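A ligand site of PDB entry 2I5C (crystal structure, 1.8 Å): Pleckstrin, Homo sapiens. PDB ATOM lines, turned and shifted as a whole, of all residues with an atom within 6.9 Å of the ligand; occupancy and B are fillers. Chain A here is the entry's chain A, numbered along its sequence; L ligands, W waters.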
ATOM      1  N   LYS A  15      15.820  -8.371  -8.866  1.00  0.00           N
ATOM      2  CA  LYS A  15      16.072  -9.530  -7.960  1.00  0.00           C
ATOM      3  C   LYS A  15      15.881 -10.783  -8.810  1.00  0.00           C
ATOM      4  O   LYS A  15      14.847 -10.912  -9.531  1.00  0.00           O
ATOM      5  CB  LYS A  15      15.043  -9.501  -6.860  1.00  0.00           C
ATOM      6  CG  LYS A  15      15.111 -10.713  -5.874  1.00  0.00           C
ATOM      7  CD  LYS A  15      14.193 -10.328  -4.632  1.00  0.00           C
ATOM      8  CE  LYS A  15      13.852 -11.468  -3.790  1.00  0.00           C
ATOM      9  NZ  LYS A  15      12.795 -12.315  -4.494  1.00  0.00           N
ATOM     10  N   GLN A  16      16.813 -11.739  -8.716  1.00  0.00           N
ATOM     11  CA  GLN A  16      16.698 -12.956  -9.508  1.00  0.00           C
ATOM     12  C   GLN A  16      15.868 -14.015  -8.810  1.00  0.00           C
ATOM     13  O   GLN A  16      15.907 -14.169  -7.574  1.00  0.00           O
ATOM     14  CB  GLN A  16      18.127 -13.512  -9.770  1.00  0.00           C
ATOM     15  CG  GLN A  16      18.111 -14.606 -10.837  1.00  0.00           C
ATOM     16  CD  GLN A  16      19.507 -14.991 -11.266  1.00  0.00           C
ATOM     17  OE1 GLN A  16      19.804 -15.039 -12.452  1.00  0.00           O
ATOM     18  NE2 GLN A  16      20.364 -15.228 -10.305  1.00  0.00           N
ATOM     19  N   GLY A  17      15.094 -14.781  -9.580  1.00  0.00           N
ATOM     20  CA  GLY A  17      14.262 -15.822  -8.988  1.00  0.00           C
ATOM     21  C   GLY A  17      15.127 -17.003  -8.610  1.00  0.00           C
ATOM     22  O   GLY A  17      16.184 -17.119  -9.100  1.00  0.00           O
ATOM     23  N   HIS A  18      14.663 -17.866  -7.695  1.00  0.00           N
ATOM     24  CA  HIS A  18      15.474 -18.915  -7.174  1.00  0.00           C
ATOM     25  C   HIS A  18      15.547 -20.107  -8.107  1.00  0.00           C
ATOM     26  O   HIS A  18      16.581 -20.700  -8.256  1.00  0.00           O
ATOM     27  CB  HIS A  18      14.964 -19.343  -5.769  1.00  0.00           C
ATOM     28  CG  HIS A  18      14.900 -18.190  -4.827  1.00  0.00           C
ATOM     29  ND1 HIS A  18      16.043 -17.570  -4.354  1.00  0.00           N
ATOM     30  CD2 HIS A  18      13.853 -17.547  -4.269  1.00  0.00           C
ATOM     31  CE1 HIS A  18      15.691 -16.578  -3.542  1.00  0.00           C
ATOM     32  NE2 HIS A  18      14.363 -16.543  -3.476  1.00  0.00           N
ATOM     33  N   ARG A  19      14.453 -20.423  -8.777  1.00  0.00           N
ATOM     34  CA  ARG A  19      14.362 -21.647  -9.614  1.00  0.00           C
ATOM     35  C   ARG A  19      14.496 -21.260 -11.070  1.00  0.00           C
ATOM     36  O   ARG A  19      15.130 -21.993 -11.837  1.00  0.00           O
ATOM     37  CB  ARG A  19      13.021 -22.362  -9.444  1.00  0.00           C
ATOM     38  CG  ARG A  19      12.926 -23.298  -8.166  1.00  0.00           C
ATOM     39  CD  ARG A  19      11.489 -23.844  -8.054  1.00  0.00           C
ATOM     40  NE  ARG A  19      11.438 -24.990  -7.101  1.00  0.00           N
ATOM     41  CZ  ARG A  19      11.415 -24.805  -5.786  1.00  0.00           C
ATOM     42  NH1 ARG A  19      11.397 -23.562  -5.274  1.00  0.00           N
ATOM     43  NH2 ARG A  19      11.388 -25.857  -4.982  1.00  0.00           N
ATOM     44  N   ARG A  20      13.838 -20.174 -11.470  1.00  0.00           N
ATOM     45  CA  ARG A  20      13.753 -19.866 -12.896  1.00  0.00           C
ATOM     46  C   ARG A  20      14.742 -18.798 -13.401  1.00  0.00           C
ATOM     47  O   ARG A  20      14.812 -18.538 -14.617  1.00  0.00           O
ATOM     48  CB  ARG A  20      12.295 -19.557 -13.311  1.00  0.00           C
ATOM     49  CG  ARG A  20      11.281 -20.742 -13.296  1.00  0.00           C
ATOM     50  CD  ARG A  20       9.825 -20.251 -13.459  1.00  0.00           C
ATOM     51  NE  ARG A  20       8.932 -21.394 -13.331  1.00  0.00           N
ATOM     52  CZ  ARG A  20       8.511 -21.844 -12.151  1.00  0.00           C
ATOM     53  NH1 ARG A  20       8.862 -21.175 -11.008  1.00  0.00           N
ATOM     54  NH2 ARG A  20       7.777 -22.953 -12.136  1.00  0.00           N
ATOM     55  N   LYS A  21      15.512 -18.172 -12.514  1.00  0.00           N
ATOM     56  CA  LYS A  21      16.601 -17.241 -12.950  1.00  0.00           C
ATOM     57  C   LYS A  21      16.250 -15.954 -13.694  1.00  0.00           C
ATOM     58  O   LYS A  21      17.098 -15.356 -14.317  1.00  0.00           O
ATOM     59  CB  LYS A  21      17.692 -17.935 -13.762  1.00  0.00           C
ATOM     60  CG  LYS A  21      18.236 -19.225 -13.117  1.00  0.00           C
ATOM     61  CD  LYS A  21      18.904 -19.004 -11.781  1.00  0.00           C
ATOM     62  CE  LYS A  21      19.439 -20.339 -11.263  1.00  0.00           C
ATOM     63  NZ  LYS A  21      19.287 -20.332  -9.754  1.00  0.00           N
ATOM     64  N   ASN A  22      14.953 -15.630 -13.732  1.00  0.00           N
ATOM     65  CA  ASN A  22      14.502 -14.431 -14.311  1.00  0.00           C
ATOM     66  C   ASN A  22      14.644 -13.314 -13.319  1.00  0.00           C
ATOM     67  O   ASN A  22      14.670 -13.559 -12.102  1.00  0.00           O
ATOM     68  CB  ASN A  22      13.054 -14.636 -14.755  1.00  0.00           C
ATOM     69  CG  ASN A  22      12.949 -15.617 -15.928  1.00  0.00           C
ATOM     70  OD1 ASN A  22      12.138 -16.552 -15.908  1.00  0.00           O
ATOM     71  ND2 ASN A  22      13.800 -15.402 -16.963  1.00  0.00           N
ATOM     72  N   LYS A  24      13.298  -9.649 -11.746  1.00  0.00           N
ATOM     73  CA  LYS A  24      12.117  -8.831 -11.550  1.00  0.00           C
ATOM     74  C   LYS A  24      12.490  -7.582 -10.808  1.00  0.00           C
ATOM     75  O   LYS A  24      13.257  -7.638  -9.861  1.00  0.00           O
ATOM     76  CB  LYS A  24      11.053  -9.604 -10.726  1.00  0.00           C
ATOM     77  CG  LYS A  24      10.570 -10.916 -11.442  1.00  0.00           C
ATOM     78  CD  LYS A  24       9.466 -11.589 -10.607  1.00  0.00           C
ATOM     79  CE  LYS A  24       8.124 -11.442 -11.359  1.00  0.00           C
ATOM     80  NZ  LYS A  24       6.914 -12.007 -10.663  1.00  0.00           N
ATOM     81  N   VAL A  25      11.911  -6.454 -11.217  1.00  0.00           N
ATOM     82  CA  VAL A  25      12.124  -5.223 -10.438  1.00  0.00           C
ATOM     83  C   VAL A  25      11.344  -5.341  -9.113  1.00  0.00           C
ATOM     84  O   VAL A  25      10.130  -5.676  -9.124  1.00  0.00           O
ATOM     85  CB  VAL A  25      11.648  -3.958 -11.181  1.00  0.00           C
ATOM     86  CG1 VAL A  25      11.922  -2.765 -10.322  1.00  0.00           C
ATOM     87  CG2 VAL A  25      12.399  -3.813 -12.510  1.00  0.00           C
ATOM     88  N   ARG A  26      12.009  -5.067  -7.992  1.00  0.00           N
ATOM     89  CA  ARG A  26      11.330  -4.898  -6.729  1.00  0.00           C
ATOM     90  C   ARG A  26      11.742  -3.607  -6.057  1.00  0.00           C
ATOM     91  O   ARG A  26      12.852  -3.107  -6.304  1.00  0.00           O
ATOM     92  CB  ARG A  26      11.666  -6.069  -5.734  1.00  0.00           C
ATOM     93  CG  ARG A  26      10.656  -7.305  -5.857  1.00  0.00           C
ATOM     94  CD  ARG A  26      10.852  -8.181  -7.037  1.00  0.00           C
ATOM     95  NE  ARG A  26       9.751  -9.178  -7.072  1.00  0.00           N
ATOM     96  CZ  ARG A  26       8.621  -9.023  -7.750  1.00  0.00           C
ATOM     97  NH1 ARG A  26       8.352  -7.887  -8.435  1.00  0.00           N
ATOM     98  NH2 ARG A  26       7.703  -9.983  -7.716  1.00  0.00           N
ATOM     99  N   TYR A  39      10.843  -6.242   0.589  1.00  0.00           N
ATOM    100  CA  TYR A  39      10.787  -5.886  -0.837  1.00  0.00           C
ATOM    101  C   TYR A  39       9.321  -6.055  -1.269  1.00  0.00           C
ATOM    102  O   TYR A  39       8.578  -6.918  -0.682  1.00  0.00           O
ATOM    103  CB  TYR A  39      11.805  -6.775  -1.645  1.00  0.00           C
ATOM    104  CG  TYR A  39      11.722  -8.274  -1.376  1.00  0.00           C
ATOM    105  CD1 TYR A  39      10.807  -9.068  -2.074  1.00  0.00           C
ATOM    106  CD2 TYR A  39      12.477  -8.856  -0.351  1.00  0.00           C
ATOM    107  CE1 TYR A  39      10.689 -10.470  -1.778  1.00  0.00           C
ATOM    108  CE2 TYR A  39      12.432 -10.236  -0.083  1.00  0.00           C
ATOM    109  CZ  TYR A  39      11.533 -11.040  -0.776  1.00  0.00           C
ATOM    110  OH  TYR A  39      11.457 -12.393  -0.440  1.00  0.00           O
ATOM    111  N   TYR A  40       8.904  -5.258  -2.279  1.00  0.00           N
ATOM    112  CA  TYR A  40       7.524  -5.064  -2.627  1.00  0.00           C
ATOM    113  C   TYR A  40       7.413  -5.057  -4.131  1.00  0.00           C
ATOM    114  O   TYR A  40       8.414  -4.754  -4.803  1.00  0.00           O
ATOM    115  CB  TYR A  40       7.087  -3.661  -2.143  1.00  0.00           C
ATOM    116  CG  TYR A  40       7.255  -3.470  -0.625  1.00  0.00           C
ATOM    117  CD1 TYR A  40       8.503  -3.108  -0.064  1.00  0.00           C
ATOM    118  CD2 TYR A  40       6.166  -3.561   0.220  1.00  0.00           C
ATOM    119  CE1 TYR A  40       8.679  -2.922   1.279  1.00  0.00           C
ATOM    120  CE2 TYR A  40       6.339  -3.406   1.626  1.00  0.00           C
ATOM    121  CZ  TYR A  40       7.593  -3.081   2.135  1.00  0.00           C
ATOM    122  OH  TYR A  40       7.750  -2.883   3.486  1.00  0.00           O
ATOM    123  N   LEU A  49       6.231  -8.498  -0.375  1.00  0.00           N
ATOM    124  CA  LEU A  49       6.389  -9.819  -0.935  1.00  0.00           C
ATOM    125  C   LEU A  49       7.232 -10.722  -0.030  1.00  0.00           C
ATOM    126  O   LEU A  49       7.061 -11.965  -0.074  1.00  0.00           O
ATOM    127  CB  LEU A  49       7.101  -9.717  -2.268  1.00  0.00           C
ATOM    128  CG  LEU A  49       6.294  -9.028  -3.374  1.00  0.00           C
ATOM    129  CD1 LEU A  49       7.151  -9.016  -4.716  1.00  0.00           C
ATOM    130  CD2 LEU A  49       4.853  -9.729  -3.526  1.00  0.00           C
ATOM    131  N   GLY A  50       8.126 -10.106   0.727  1.00  0.00           N
ATOM    132  CA  GLY A  50       9.027 -10.862   1.550  1.00  0.00           C
ATOM    133  C   GLY A  50       9.938  -9.932   2.330  1.00  0.00           C
ATOM    134  O   GLY A  50       9.899  -8.691   2.158  1.00  0.00           O
ATOM    135  N   ALA A  51      10.750 -10.531   3.195  1.00  0.00           N
ATOM    136  CA  ALA A  51      11.771  -9.753   3.878  1.00  0.00           C
ATOM    137  C   ALA A  51      12.991 -10.589   4.101  1.00  0.00           C
ATOM    138  O   ALA A  51      12.899 -11.840   4.381  1.00  0.00           O
ATOM    139  CB  ALA A  51      11.229  -9.245   5.249  1.00  0.00           C
ATOM    140  N   VAL A  85      20.489 -18.644   2.728  1.00  0.00           N
ATOM    141  CA  VAL A  85      19.773 -18.336   1.490  1.00  0.00           C
ATOM    142  C   VAL A  85      20.536 -17.285   0.688  1.00  0.00           C
ATOM    143  O   VAL A  85      21.057 -16.286   1.262  1.00  0.00           O
ATOM    144  CB  VAL A  85      18.361 -17.766   1.835  1.00  0.00           C
ATOM    145  CG1 VAL A  85      17.649 -17.361   0.583  1.00  0.00           C
ATOM    146  CG2 VAL A  85      17.574 -18.894   2.533  1.00  0.00           C
ATOM    147  N   TYR A  87      20.530 -14.407  -2.220  1.00  0.00           N
ATOM    148  CA  TYR A  87      19.697 -13.502  -3.042  1.00  0.00           C
ATOM    149  C   TYR A  87      20.639 -12.786  -4.005  1.00  0.00           C
ATOM    150  O   TYR A  87      21.620 -12.116  -3.611  1.00  0.00           O
ATOM    151  CB  TYR A  87      19.018 -12.490  -2.138  1.00  0.00           C
ATOM    152  CG  TYR A  87      17.999 -13.075  -1.213  1.00  0.00           C
ATOM    153  CD1 TYR A  87      18.318 -13.502   0.106  1.00  0.00           C
ATOM    154  CD2 TYR A  87      16.669 -13.228  -1.658  1.00  0.00           C
ATOM    155  CE1 TYR A  87      17.317 -14.089   0.939  1.00  0.00           C
ATOM    156  CE2 TYR A  87      15.702 -13.861  -0.860  1.00  0.00           C
ATOM    157  CZ  TYR A  87      16.040 -14.243   0.449  1.00  0.00           C
ATOM    158  OH  TYR A  87      15.041 -14.756   1.234  1.00  0.00           O
HETATM  159  O1  LIG L   1      10.911 -14.930  -7.825  1.00  0.00           O
HETATM  160  C1  LIG L   1      10.760 -15.648  -6.595  1.00  0.00           C
HETATM  161  C2  LIG L   1       9.706 -14.961  -5.728  1.00  0.00           C
HETATM  162  O2  LIG L   1      10.210 -13.659  -5.477  1.00  0.00           O
HETATM  163  P1  LIG L   1       9.282 -12.383  -5.185  1.00  0.00           P
HETATM  164  O3  LIG L   1       8.760 -12.720  -3.798  1.00  0.00           O
HETATM  165  O4  LIG L   1      10.288 -11.251  -5.305  1.00  0.00           O
HETATM  166  O5  LIG L   1       8.149 -12.382  -6.201  1.00  0.00           O
HETATM  167  C3  LIG L   1      10.328 -17.102  -6.901  1.00  0.00           C
HETATM  168  O6  LIG L   1      11.359 -17.775  -7.643  1.00  0.00           O
HETATM  169  P2  LIG L   1      11.164 -18.516  -9.082  1.00  0.00           P
HETATM  170  O7  LIG L   1      12.421 -18.380  -9.907  1.00  0.00           O
HETATM  171  O8  LIG L   1       9.896 -17.933  -9.617  1.00  0.00           O
HETATM  172  O9  LIG L   1      10.904 -19.921  -8.592  1.00  0.00           O
HETATM  173  C4  LIG L   1       9.961 -17.943  -5.625  1.00  0.00           C
HETATM  174  O10 LIG L   1       9.242 -19.119  -5.986  1.00  0.00           O
HETATM  175  P3  LIG L   1       9.735 -20.602  -5.538  1.00  0.00           P
HETATM  176  O11 LIG L   1      10.902 -20.835  -6.380  1.00  0.00           O
HETATM  177  O12 LIG L   1      10.160 -20.647  -4.089  1.00  0.00           O
HETATM  178  O13 LIG L   1       8.516 -21.475  -5.755  1.00  0.00           O
HETATM  179  C5  LIG L   1       8.957 -17.163  -4.767  1.00  0.00           C
HETATM  180  O14 LIG L   1       8.686 -17.947  -3.594  1.00  0.00           O
HETATM  181  P4  LIG L   1       7.249 -17.929  -2.860  1.00  0.00           P
HETATM  182  O15 LIG L   1       7.050 -16.491  -2.395  1.00  0.00           O
HETATM  183  O16 LIG L   1       6.254 -18.431  -3.867  1.00  0.00           O
HETATM  184  O17 LIG L   1       7.375 -18.911  -1.734  1.00  0.00           O
HETATM  185  C6  LIG L   1       9.480 -15.757  -4.424  1.00  0.00           C
HETATM  186  O18 LIG L   1      10.729 -15.920  -3.715  1.00  0.00           O
HETATM  187  P5  LIG L   1      11.121 -15.094  -2.409  1.00  0.00           P
HETATM  188  O19 LIG L   1      10.294 -13.830  -2.178  1.00  0.00           O
HETATM  189  O20 LIG L   1      10.988 -15.981  -1.214  1.00  0.00           O
HETATM  190  O21 LIG L   1      12.472 -14.601  -2.793  1.00  0.00           O
HETATM  191  O   HOH W   1       7.335 -18.757  -8.470  1.00  0.00           O
HETATM  192  O   HOH W   2       5.712 -13.251  -5.031  1.00  0.00           O
HETATM  193  O   HOH W   3      12.395 -16.250 -11.768  1.00  0.00           O
HETATM  194  O   HOH W   4       6.243 -20.041  -6.328  1.00  0.00           O
HETATM  195  O   HOH W   5       5.625 -15.768  -5.793  1.00  0.00           O
HETATM  196  O   HOH W   6       7.648 -13.337  -8.518  1.00  0.00           O
HETATM  197  O   HOH W   7      12.441 -12.618  -7.442  1.00  0.00           O
HETATM  198  O   HOH W   8      12.575 -13.994   1.033  1.00  0.00           O
HETATM  199  O   HOH W   9       9.312 -14.752  -9.901  1.00  0.00           O
HETATM  200  O   HOH W  10       3.854 -18.754  -3.553  1.00  0.00           O
HETATM  201  O   HOH W  11       8.519 -14.406   0.331  1.00  0.00           O
HETATM  202  O   HOH W  12      13.452 -16.670   0.074  1.00  0.00           O
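N of Arg 20 lies within hydrogen-bond range of O7 of the ligand, at 2.8 Å. O11 of the ligand lies within salt-bridge range of NH1 of Arg 19, 3.0 Å away. A ring nitrogen (NE2) of His 18 lies within hydrogen-bond range of an oxygen (O21) of the ligand (2.8 Å). OH of Tyr 39 lies within hydrogen-bond range of O19 of the ligand, 2.5 Å away. O4 of the ligand is in salt-bridge range of NE of Arg 26, 2.8 Å away. An oxygen (O4) of the ligand is in salt-bridge range of the side-chain amino group of Lys 15 (2.8 Å). O7 of the ligand is in hydrogen-bond range of N of His 18 (3.2 Å). The guanidinium group of Arg 20 is in salt-bridge range of an oxygen (O9) of the ligand (3.4 Å). The backbone NH (N) of Arg 19 sits at hydrogen-bond distance from an oxygen (O7) of the ligand (3.1 Å).
The backbone NH of Gly 17 lies within hydrogen-bond range of the backbone carbonyl oxygen of Asn 22. N of Leu 49 is in hydrogen-bond range of O of Tyr 39, 2.8 Å away. The backbone NH (N) of Tyr 39 is in hydrogen-bond range of the backbone carbonyl oxygen (O) of Gly 50, 3.1 Å away. The backbone carbonyl oxygen (O) of His 18 lies within hydrogen-bond range of the side-chain amino group (NZ) of Lys 21. The backbone NH (N) of Lys 15 lies within hydrogen-bond range of the backbone carbonyl oxygen (O) of Lys 24, at 2.8 Å.
Merely in contact with the ligand: Gly 17, Leu 49 and Tyr 87. Hydrophobic or aromatic side chains that line the ligand: His 18, Tyr 39, Leu 49 and Tyr 87. Within 4 Å of the ligand: Lys 15, Gly 17, His 18, Arg 19, Arg 20, Arg 26, Tyr 39, Leu 49 and Tyr 87.
Water W6 lies within hydrogen-bond range of O5 of the ligand (2.6 Å), NZ of Lys 24 (2.6 Å) and NH2 of Arg 26 (3.4 Å). Water W7 bridges O1 of the ligand (2.8 Å) and NZ of Lys 15 (3.0 Å). Water W3 bridges O7 of the ligand (2.8 Å) and N of Asn 22 (3.3 Å). Water W12 lies within hydrogen-bond range of the side-chain hydroxyl (OH) of Tyr 87 (2.7 Å) and an oxygen (O20) of the ligand (2.9 Å). Water W11 lies within hydrogen-bond range of the backbone carbonyl oxygen of Leu 49 and an oxygen (O19) of the ligand. Water W8 lies within hydrogen-bond range of the side-chain hydroxyl of Tyr 39 (2.4 Å), the side-chain hydroxyl of Tyr 87 (2.6 Å) and an oxygen (O20) of the ligand (3.4 Å).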
